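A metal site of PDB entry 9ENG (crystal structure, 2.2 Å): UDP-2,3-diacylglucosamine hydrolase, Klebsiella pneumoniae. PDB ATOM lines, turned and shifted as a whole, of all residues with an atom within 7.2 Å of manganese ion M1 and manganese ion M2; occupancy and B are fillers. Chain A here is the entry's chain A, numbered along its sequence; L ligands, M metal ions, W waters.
ND2 of Asn 79 sits at hydrogen-bond distance from O3 of the ligand, 3.0 Å away.
OE1 of Glu 44 is in hydrogen-bond range of ND1 of His 10.
OD2 of Asp 8 sits at hydrogen-bond distance from N of His 195 (2.7 Å).
The backbone carbonyl oxygen of Asp 41 sits at hydrogen-bond distance from the backbone NH of Leu 9 (3.0 Å).
O of Leu 39 sits at hydrogen-bond distance from ND1 of His 114 (2.6 Å).
The backbone NH of Arg 80 is in hydrogen-bond range of the side-chain carboxylate of Asp 41 (3.2 Å).
OD1 of Asp 81 is in hydrogen-bond range of N of Asp 41 (3.0 Å).
O of Gly 40 sits at hydrogen-bond distance from N of Asp 8 (2.9 Å).
N of Gly 194 sits at hydrogen-bond distance from O of His 114, 2.8 Å away.
The nearest printed residue that does not touch manganese ion M1 is His 10 (4.9 Å).
Manganese ion M1 is bound by OD2 of Asp 41 (2.1 Å), OD1 of Asn 79 (2.2 Å), water W1 (2.2 Å), ND1 of His 195 (2.2 Å) and NE2 of His 114 (2.2 Å).
Manganese ion M1 has five donor atoms within binding distance.
Manganese ion M2 is bound by OD1 of Asp 8, at 2.1 Å.
Water W1 is bound to manganese ion M2 (2.1 Å).
NE2 of His 10 binds manganese ion M2, at 2.2 Å.
OD2 of Asp 41 is bound to manganese ion M2, 2.2 Å away.
A ring nitrogen (NE2) of His 197 is bound to manganese ion M2, 2.2 Å away.
Manganese ion M2 has five donor atoms within binding distance.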
ATOM      1  N   ALA A   7      10.845  26.123  12.363  1.00  0.00           N
ATOM      2  CA  ALA A   7      11.217  24.939  11.614  1.00  0.00           C
ATOM      3  C   ALA A   7      10.065  23.956  11.663  1.00  0.00           C
ATOM      4  O   ALA A   7       9.159  24.102  12.483  1.00  0.00           O
ATOM      5  CB  ALA A   7      12.483  24.345  12.147  1.00  0.00           C
ATOM      6  N   ASP A   8      10.071  22.966  10.773  1.00  0.00           N
ATOM      7  CA  ASP A   8       9.263  21.768  10.974  1.00  0.00           C
ATOM      8  C   ASP A   8       7.779  22.078  10.874  1.00  0.00           C
ATOM      9  O   ASP A   8       6.951  21.481  11.555  1.00  0.00           O
ATOM     10  CB  ASP A   8       9.659  21.085  12.282  1.00  0.00           C
ATOM     11  CG  ASP A   8      11.074  20.525  12.219  1.00  0.00           C
ATOM     12  OD1 ASP A   8      11.276  19.633  11.424  1.00  0.00           O
ATOM     13  OD2 ASP A   8      11.974  21.033  12.913  1.00  0.00           O
ATOM     14  N   LEU A   9       7.430  22.991   9.965  1.00  0.00           N
ATOM     15  CA  LEU A   9       6.037  23.253   9.668  1.00  0.00           C
ATOM     16  C   LEU A   9       5.386  22.107   8.873  1.00  0.00           C
ATOM     17  O   LEU A   9       4.169  21.925   8.947  1.00  0.00           O
ATOM     18  CB  LEU A   9       5.967  24.573   8.903  1.00  0.00           C
ATOM     19  CG  LEU A   9       6.265  25.816   9.760  1.00  0.00           C
ATOM     20  CD1 LEU A   9       7.754  26.145   9.774  1.00  0.00           C
ATOM     21  CD2 LEU A   9       5.464  26.990   9.250  1.00  0.00           C
ATOM     22  N   HIS A  10       6.194  21.346   8.112  1.00  0.00           N
ATOM     23  CA  HIS A  10       5.712  20.229   7.296  1.00  0.00           C
ATOM     24  C   HIS A  10       4.438  20.571   6.547  1.00  0.00           C
ATOM     25  O   HIS A  10       3.436  19.869   6.642  1.00  0.00           O
ATOM     26  CB  HIS A  10       5.532  18.971   8.156  1.00  0.00           C
ATOM     27  CG  HIS A  10       6.815  18.432   8.694  1.00  0.00           C
ATOM     28  ND1 HIS A  10       7.542  17.415   8.118  1.00  0.00           N
ATOM     29  CD2 HIS A  10       7.523  18.828   9.762  1.00  0.00           C
ATOM     30  CE1 HIS A  10       8.637  17.194   8.824  1.00  0.00           C
ATOM     31  NE2 HIS A  10       8.631  18.033   9.841  1.00  0.00           N
ATOM     32  N   LEU A  39      14.483  26.944   9.651  1.00  0.00           N
ATOM     33  CA  LEU A  39      15.528  25.928   9.734  1.00  0.00           C
ATOM     34  C   LEU A  39      15.049  24.561   9.257  1.00  0.00           C
ATOM     35  O   LEU A  39      15.343  23.550   9.891  1.00  0.00           O
ATOM     36  CB  LEU A  39      16.036  25.853  11.176  1.00  0.00           C
ATOM     37  CG  LEU A  39      16.434  27.185  11.810  1.00  0.00           C
ATOM     38  CD1 LEU A  39      17.164  26.935  13.116  1.00  0.00           C
ATOM     39  CD2 LEU A  39      17.286  28.010  10.862  1.00  0.00           C
ATOM     40  N   GLY A  40      14.323  24.525   8.118  1.00  0.00           N
ATOM     41  CA  GLY A  40      14.109  23.308   7.359  1.00  0.00           C
ATOM     42  C   GLY A  40      12.779  22.641   7.704  1.00  0.00           C
ATOM     43  O   GLY A  40      12.195  22.941   8.741  1.00  0.00           O
ATOM     44  N   ASP A  41      12.338  21.737   6.825  1.00  0.00           N
ATOM     45  CA  ASP A  41      11.042  21.084   6.881  1.00  0.00           C
ATOM     46  C   ASP A  41       9.936  22.148   6.899  1.00  0.00           C
ATOM     47  O   ASP A  41       8.927  22.031   7.601  1.00  0.00           O
ATOM     48  CB  ASP A  41      10.943  20.128   8.074  1.00  0.00           C
ATOM     49  CG  ASP A  41      11.810  18.882   7.969  1.00  0.00           C
ATOM     50  OD1 ASP A  41      12.517  18.758   6.934  1.00  0.00           O
ATOM     51  OD2 ASP A  41      11.771  18.051   8.930  1.00  0.00           O
ATOM     52  N   LEU A  42      10.094  23.157   6.065  1.00  0.00           N
ATOM     53  CA  LEU A  42       8.986  24.038   5.772  1.00  0.00           C
ATOM     54  C   LEU A  42       7.901  23.244   5.064  1.00  0.00           C
ATOM     55  O   LEU A  42       6.706  23.447   5.299  1.00  0.00           O
ATOM     56  CB  LEU A  42       9.497  25.202   4.911  1.00  0.00           C
ATOM     57  CG  LEU A  42       8.476  26.272   4.544  1.00  0.00           C
ATOM     58  CD1 LEU A  42       7.843  26.899   5.785  1.00  0.00           C
ATOM     59  CD2 LEU A  42       9.140  27.346   3.719  1.00  0.00           C
ATOM     60  N   GLU A  44       6.377  19.354   3.712  1.00  0.00           N
ATOM     61  CA  GLU A  44       6.313  17.934   4.031  1.00  0.00           C
ATOM     62  C   GLU A  44       7.078  17.109   2.978  1.00  0.00           C
ATOM     63  O   GLU A  44       7.540  16.011   3.271  1.00  0.00           O
ATOM     64  CB  GLU A  44       4.860  17.467   4.028  1.00  0.00           C
ATOM     65  CG  GLU A  44       4.666  15.974   4.310  1.00  0.00           C
ATOM     66  CD  GLU A  44       5.520  15.413   5.437  1.00  0.00           C
ATOM     67  OE1 GLU A  44       6.129  16.210   6.179  1.00  0.00           O
ATOM     68  OE2 GLU A  44       5.579  14.172   5.568  1.00  0.00           O
ATOM     69  N   GLY A  78      15.805  21.068   5.209  1.00  0.00           N
ATOM     70  CA  GLY A  78      15.641  19.890   6.030  1.00  0.00           C
ATOM     71  C   GLY A  78      15.737  18.618   5.189  1.00  0.00           C
ATOM     72  O   GLY A  78      16.048  18.688   4.013  1.00  0.00           O
ATOM     73  N   ASN A  79      15.487  17.486   5.839  1.00  0.00           N
ATOM     74  CA  ASN A  79      15.509  16.193   5.188  1.00  0.00           C
ATOM     75  C   ASN A  79      14.303  16.058   4.236  1.00  0.00           C
ATOM     76  O   ASN A  79      14.351  15.273   3.295  1.00  0.00           O
ATOM     77  CB  ASN A  79      15.544  15.065   6.229  1.00  0.00           C
ATOM     78  CG  ASN A  79      14.387  15.091   7.207  1.00  0.00           C
ATOM     79  OD1 ASN A  79      14.359  15.921   8.111  1.00  0.00           O
ATOM     80  ND2 ASN A  79      13.447  14.178   7.059  1.00  0.00           N
ATOM     81  N   ARG A  80      13.213  16.802   4.510  1.00  0.00           N
ATOM     82  CA  ARG A  80      11.993  16.662   3.732  1.00  0.00           C
ATOM     83  C   ARG A  80      12.089  17.500   2.462  1.00  0.00           C
ATOM     84  O   ARG A  80      11.544  17.096   1.438  1.00  0.00           O
ATOM     85  CB  ARG A  80      10.716  17.052   4.488  1.00  0.00           C
ATOM     86  CG  ARG A  80      10.443  16.257   5.777  1.00  0.00           C
ATOM     87  CD  ARG A  80      10.277  14.750   5.658  1.00  0.00           C
ATOM     88  NE  ARG A  80       9.301  14.431   4.630  1.00  0.00           N
ATOM     89  CZ  ARG A  80       9.002  13.211   4.217  1.00  0.00           C
ATOM     90  NH1 ARG A  80       9.412  12.160   4.886  1.00  0.00           N
ATOM     91  NH2 ARG A  80       8.250  13.069   3.129  1.00  0.00           N
ATOM     92  N   ASP A  81      12.760  18.660   2.538  1.00  0.00           N
ATOM     93  CA  ASP A  81      12.681  19.674   1.496  1.00  0.00           C
ATOM     94  C   ASP A  81      14.069  20.120   1.006  1.00  0.00           C
ATOM     95  O   ASP A  81      14.225  21.249   0.522  1.00  0.00           O
ATOM     96  CB  ASP A  81      11.827  20.863   1.934  1.00  0.00           C
ATOM     97  CG  ASP A  81      12.111  21.424   3.321  1.00  0.00           C
ATOM     98  OD1 ASP A  81      13.099  20.991   3.987  1.00  0.00           O
ATOM     99  OD2 ASP A  81      11.367  22.324   3.710  1.00  0.00           O
ATOM    100  N   HIS A 114      19.419  22.415  10.633  1.00  0.00           N
ATOM    101  CA  HIS A 114      18.130  21.756  10.683  1.00  0.00           C
ATOM    102  C   HIS A 114      18.101  20.811  11.880  1.00  0.00           C
ATOM    103  O   HIS A 114      17.079  20.686  12.554  1.00  0.00           O
ATOM    104  CB  HIS A 114      17.770  20.983   9.406  1.00  0.00           C
ATOM    105  CG  HIS A 114      16.478  20.236   9.538  1.00  0.00           C
ATOM    106  ND1 HIS A 114      15.309  20.940   9.712  1.00  0.00           N
ATOM    107  CD2 HIS A 114      16.144  18.940   9.528  1.00  0.00           C
ATOM    108  CE1 HIS A 114      14.300  20.076   9.807  1.00  0.00           C
ATOM    109  NE2 HIS A 114      14.774  18.859   9.687  1.00  0.00           N
ATOM    110  N   GLY A 115      19.212  20.095  12.055  1.00  0.00           N
ATOM    111  CA  GLY A 115      19.374  19.230  13.206  1.00  0.00           C
ATOM    112  C   GLY A 115      19.578  17.773  12.831  1.00  0.00           C
ATOM    113  O   GLY A 115      20.020  16.971  13.655  1.00  0.00           O
ATOM    114  N   ASP A 116      19.247  17.413  11.582  1.00  0.00           N
ATOM    115  CA  ASP A 116      19.288  16.020  11.183  1.00  0.00           C
ATOM    116  C   ASP A 116      20.723  15.506  11.083  1.00  0.00           C
ATOM    117  O   ASP A 116      20.948  14.304  11.236  1.00  0.00           O
ATOM    118  CB  ASP A 116      18.533  15.782   9.867  1.00  0.00           C
ATOM    119  CG  ASP A 116      19.109  16.553   8.701  1.00  0.00           C
ATOM    120  OD1 ASP A 116      19.531  15.908   7.718  1.00  0.00           O
ATOM    121  OD2 ASP A 116      19.129  17.793   8.782  1.00  0.00           O
ATOM    122  N   TYR A 125      19.567   6.492   7.935  1.00  0.00           N
ATOM    123  CA  TYR A 125      19.216   7.801   7.409  1.00  0.00           C
ATOM    124  C   TYR A 125      20.450   8.468   6.814  1.00  0.00           C
ATOM    125  O   TYR A 125      20.342   9.212   5.846  1.00  0.00           O
ATOM    126  CB  TYR A 125      18.630   8.726   8.476  1.00  0.00           C
ATOM    127  CG  TYR A 125      18.565  10.165   8.015  1.00  0.00           C
ATOM    128  CD1 TYR A 125      17.601  10.582   7.113  1.00  0.00           C
ATOM    129  CD2 TYR A 125      19.515  11.092   8.423  1.00  0.00           C
ATOM    130  CE1 TYR A 125      17.543  11.883   6.664  1.00  0.00           C
ATOM    131  CE2 TYR A 125      19.481  12.397   7.978  1.00  0.00           C
ATOM    132  CZ  TYR A 125      18.490  12.785   7.091  1.00  0.00           C
ATOM    133  OH  TYR A 125      18.412  14.060   6.622  1.00  0.00           O
ATOM    134  N   ILE A 171      11.174   9.742  15.261  1.00  0.00           N
ATOM    135  CA  ILE A 171      12.380  10.406  14.785  1.00  0.00           C
ATOM    136  C   ILE A 171      13.497  10.248  15.814  1.00  0.00           C
ATOM    137  O   ILE A 171      13.389  10.723  16.942  1.00  0.00           O
ATOM    138  CB  ILE A 171      12.072  11.893  14.495  1.00  0.00           C
ATOM    139  CG1 ILE A 171      10.972  12.042  13.439  1.00  0.00           C
ATOM    140  CG2 ILE A 171      13.331  12.655  14.121  1.00  0.00           C
ATOM    141  CD1 ILE A 171      10.526  13.478  13.252  1.00  0.00           C
ATOM    142  N   GLY A 194      15.952  22.246  14.632  1.00  0.00           N
ATOM    143  CA  GLY A 194      14.690  21.553  14.731  1.00  0.00           C
ATOM    144  C   GLY A 194      14.874  20.052  14.541  1.00  0.00           C
ATOM    145  O   GLY A 194      15.769  19.434  15.138  1.00  0.00           O
ATOM    146  N   HIS A 195      14.071  19.524  13.613  1.00  0.00           N
ATOM    147  CA  HIS A 195      14.180  18.160  13.083  1.00  0.00           C
ATOM    148  C   HIS A 195      13.698  17.101  14.065  1.00  0.00           C
ATOM    149  O   HIS A 195      13.025  16.164  13.641  1.00  0.00           O
ATOM    150  CB  HIS A 195      15.599  17.793  12.614  1.00  0.00           C
ATOM    151  CG  HIS A 195      15.634  16.401  12.113  1.00  0.00           C
ATOM    152  ND1 HIS A 195      14.902  15.949  11.032  1.00  0.00           N
ATOM    153  CD2 HIS A 195      16.254  15.327  12.637  1.00  0.00           C
ATOM    154  CE1 HIS A 195      15.115  14.639  10.899  1.00  0.00           C
ATOM    155  NE2 HIS A 195      15.933  14.238  11.863  1.00  0.00           N
ATOM    156  N   THR A 196      14.140  17.151  15.321  1.00  0.00           N
ATOM    157  CA  THR A 196      13.833  16.079  16.271  1.00  0.00           C
ATOM    158  C   THR A 196      12.384  16.152  16.763  1.00  0.00           C
ATOM    159  O   THR A 196      11.867  15.181  17.334  1.00  0.00           O
ATOM    160  CB  THR A 196      14.775  16.125  17.485  1.00  0.00           C
ATOM    161  OG1 THR A 196      14.613  17.377  18.131  1.00  0.00           O
ATOM    162  CG2 THR A 196      16.240  15.968  17.151  1.00  0.00           C
ATOM    163  N   HIS A 197      11.739  17.315  16.627  1.00  0.00           N
ATOM    164  CA  HIS A 197      10.334  17.512  16.997  1.00  0.00           C
ATOM    165  C   HIS A 197      10.118  17.462  18.516  1.00  0.00           C
ATOM    166  O   HIS A 197       8.977  17.389  18.954  1.00  0.00           O
ATOM    167  CB  HIS A 197       9.415  16.537  16.244  1.00  0.00           C
ATOM    168  CG  HIS A 197       9.337  16.772  14.775  1.00  0.00           C
ATOM    169  ND1 HIS A 197       8.407  16.159  13.958  1.00  0.00           N
ATOM    170  CD2 HIS A 197      10.031  17.603  13.981  1.00  0.00           C
ATOM    171  CE1 HIS A 197       8.544  16.623  12.726  1.00  0.00           C
ATOM    172  NE2 HIS A 197       9.519  17.521  12.724  1.00  0.00           N
ATOM    173  N   ALA A 218       7.686  20.864  16.016  1.00  0.00           N
ATOM    174  CA  ALA A 218       6.848  20.776  14.823  1.00  0.00           C
ATOM    175  C   ALA A 218       5.545  21.552  14.987  1.00  0.00           C
ATOM    176  O   ALA A 218       5.057  21.766  16.097  1.00  0.00           O
ATOM    177  CB  ALA A 218       6.575  19.318  14.524  1.00  0.00           C
HETATM  178  C1  LIG L   1      15.447  10.337  -5.524  1.00  0.00           C
HETATM  179  C2  LIG L   1      14.323  10.751  -4.787  1.00  0.00           C
HETATM  180  C3  LIG L   1      14.322  12.021  -4.219  1.00  0.00           C
HETATM  181  C4  LIG L   1      15.464  12.764  -4.311  1.00  0.00           C
HETATM  182  C5  LIG L   1      16.554  12.303  -5.025  1.00  0.00           C
HETATM  183  C6  LIG L   1      16.582  11.089  -5.652  1.00  0.00           C
HETATM  184  N1  LIG L   1      13.235  12.484  -3.426  1.00  0.00           N
HETATM  185  C7  LIG L   1      13.091  13.894  -3.247  1.00  0.00           C
HETATM  186  C8  LIG L   1      12.293  14.111  -1.967  1.00  0.00           C
HETATM  187  C9  LIG L   1      11.947  11.918  -3.820  1.00  0.00           C
HETATM  188  C10 LIG L   1      10.963  12.053  -2.619  1.00  0.00           C
HETATM  189  N2  LIG L   1      10.918  13.489  -2.060  1.00  0.00           N
HETATM  190  S1  LIG L   1       9.962  13.713  -0.722  1.00  0.00           S
HETATM  191  C11 LIG L   1      10.693  12.815   0.558  1.00  0.00           C
HETATM  192  O1  LIG L   1       9.998  15.102  -0.390  1.00  0.00           O
HETATM  193  O2  LIG L   1       8.698  13.091  -0.994  1.00  0.00           O
HETATM  194  C12 LIG L   1      10.255  11.535   0.815  1.00  0.00           C
HETATM  195  C13 LIG L   1      10.860  10.774   1.786  1.00  0.00           C
HETATM  196  C14 LIG L   1      11.909  11.294   2.506  1.00  0.00           C
HETATM  197  C15 LIG L   1      11.773  13.329   1.265  1.00  0.00           C
HETATM  198  C16 LIG L   1      12.391  12.558   2.225  1.00  0.00           C
HETATM  199  N3  LIG L   1      12.524  10.480   3.447  1.00  0.00           N
HETATM  200  C17 LIG L   1      13.119  10.968   4.565  1.00  0.00           C
HETATM  201  O3  LIG L   1      13.129  12.177   4.793  1.00  0.00           O
HETATM  202  C18 LIG L   1      13.788   9.969   5.508  1.00  0.00           C
HETATM  203  C19 LIG L   1      14.582   8.943   4.968  1.00  0.00           C
HETATM  204  C20 LIG L   1      15.188   7.998   5.799  1.00  0.00           C
HETATM  205  C21 LIG L   1      15.006   8.052   7.168  1.00  0.00           C
HETATM  206  C22 LIG L   1      14.222   9.071   7.727  1.00  0.00           C
HETATM  207  C23 LIG L   1      13.593  10.017   6.903  1.00  0.00           C
HETATM  208  N4  LIG L   1      14.040   9.089   9.167  1.00  0.00           N
HETATM  209  S2  LIG L   1      14.421  10.412  10.088  1.00  0.00           S
HETATM  210  C24 LIG L   1      16.129  10.354  10.602  1.00  0.00           C
HETATM  211  O4  LIG L   1      14.221  11.587   9.282  1.00  0.00           O
HETATM  212  O5  LIG L   1      13.677  10.292  11.295  1.00  0.00           O
HETATM  213 CL1  LIG L   1      17.919  13.303  -5.160  1.00  0.00          CL
HETATM  214 CL2  LIG L   1      15.433   8.823  -6.345  1.00  0.00          CL
HETATM  215 MN    MN M   1      13.474  17.028   9.733  1.00  0.00          MN
HETATM  216 MN    MN M   2      10.585  17.770  10.768  1.00  0.00          MN
HETATM  217  O   HOH W   1      12.047  16.266  11.228  1.00  0.00           O
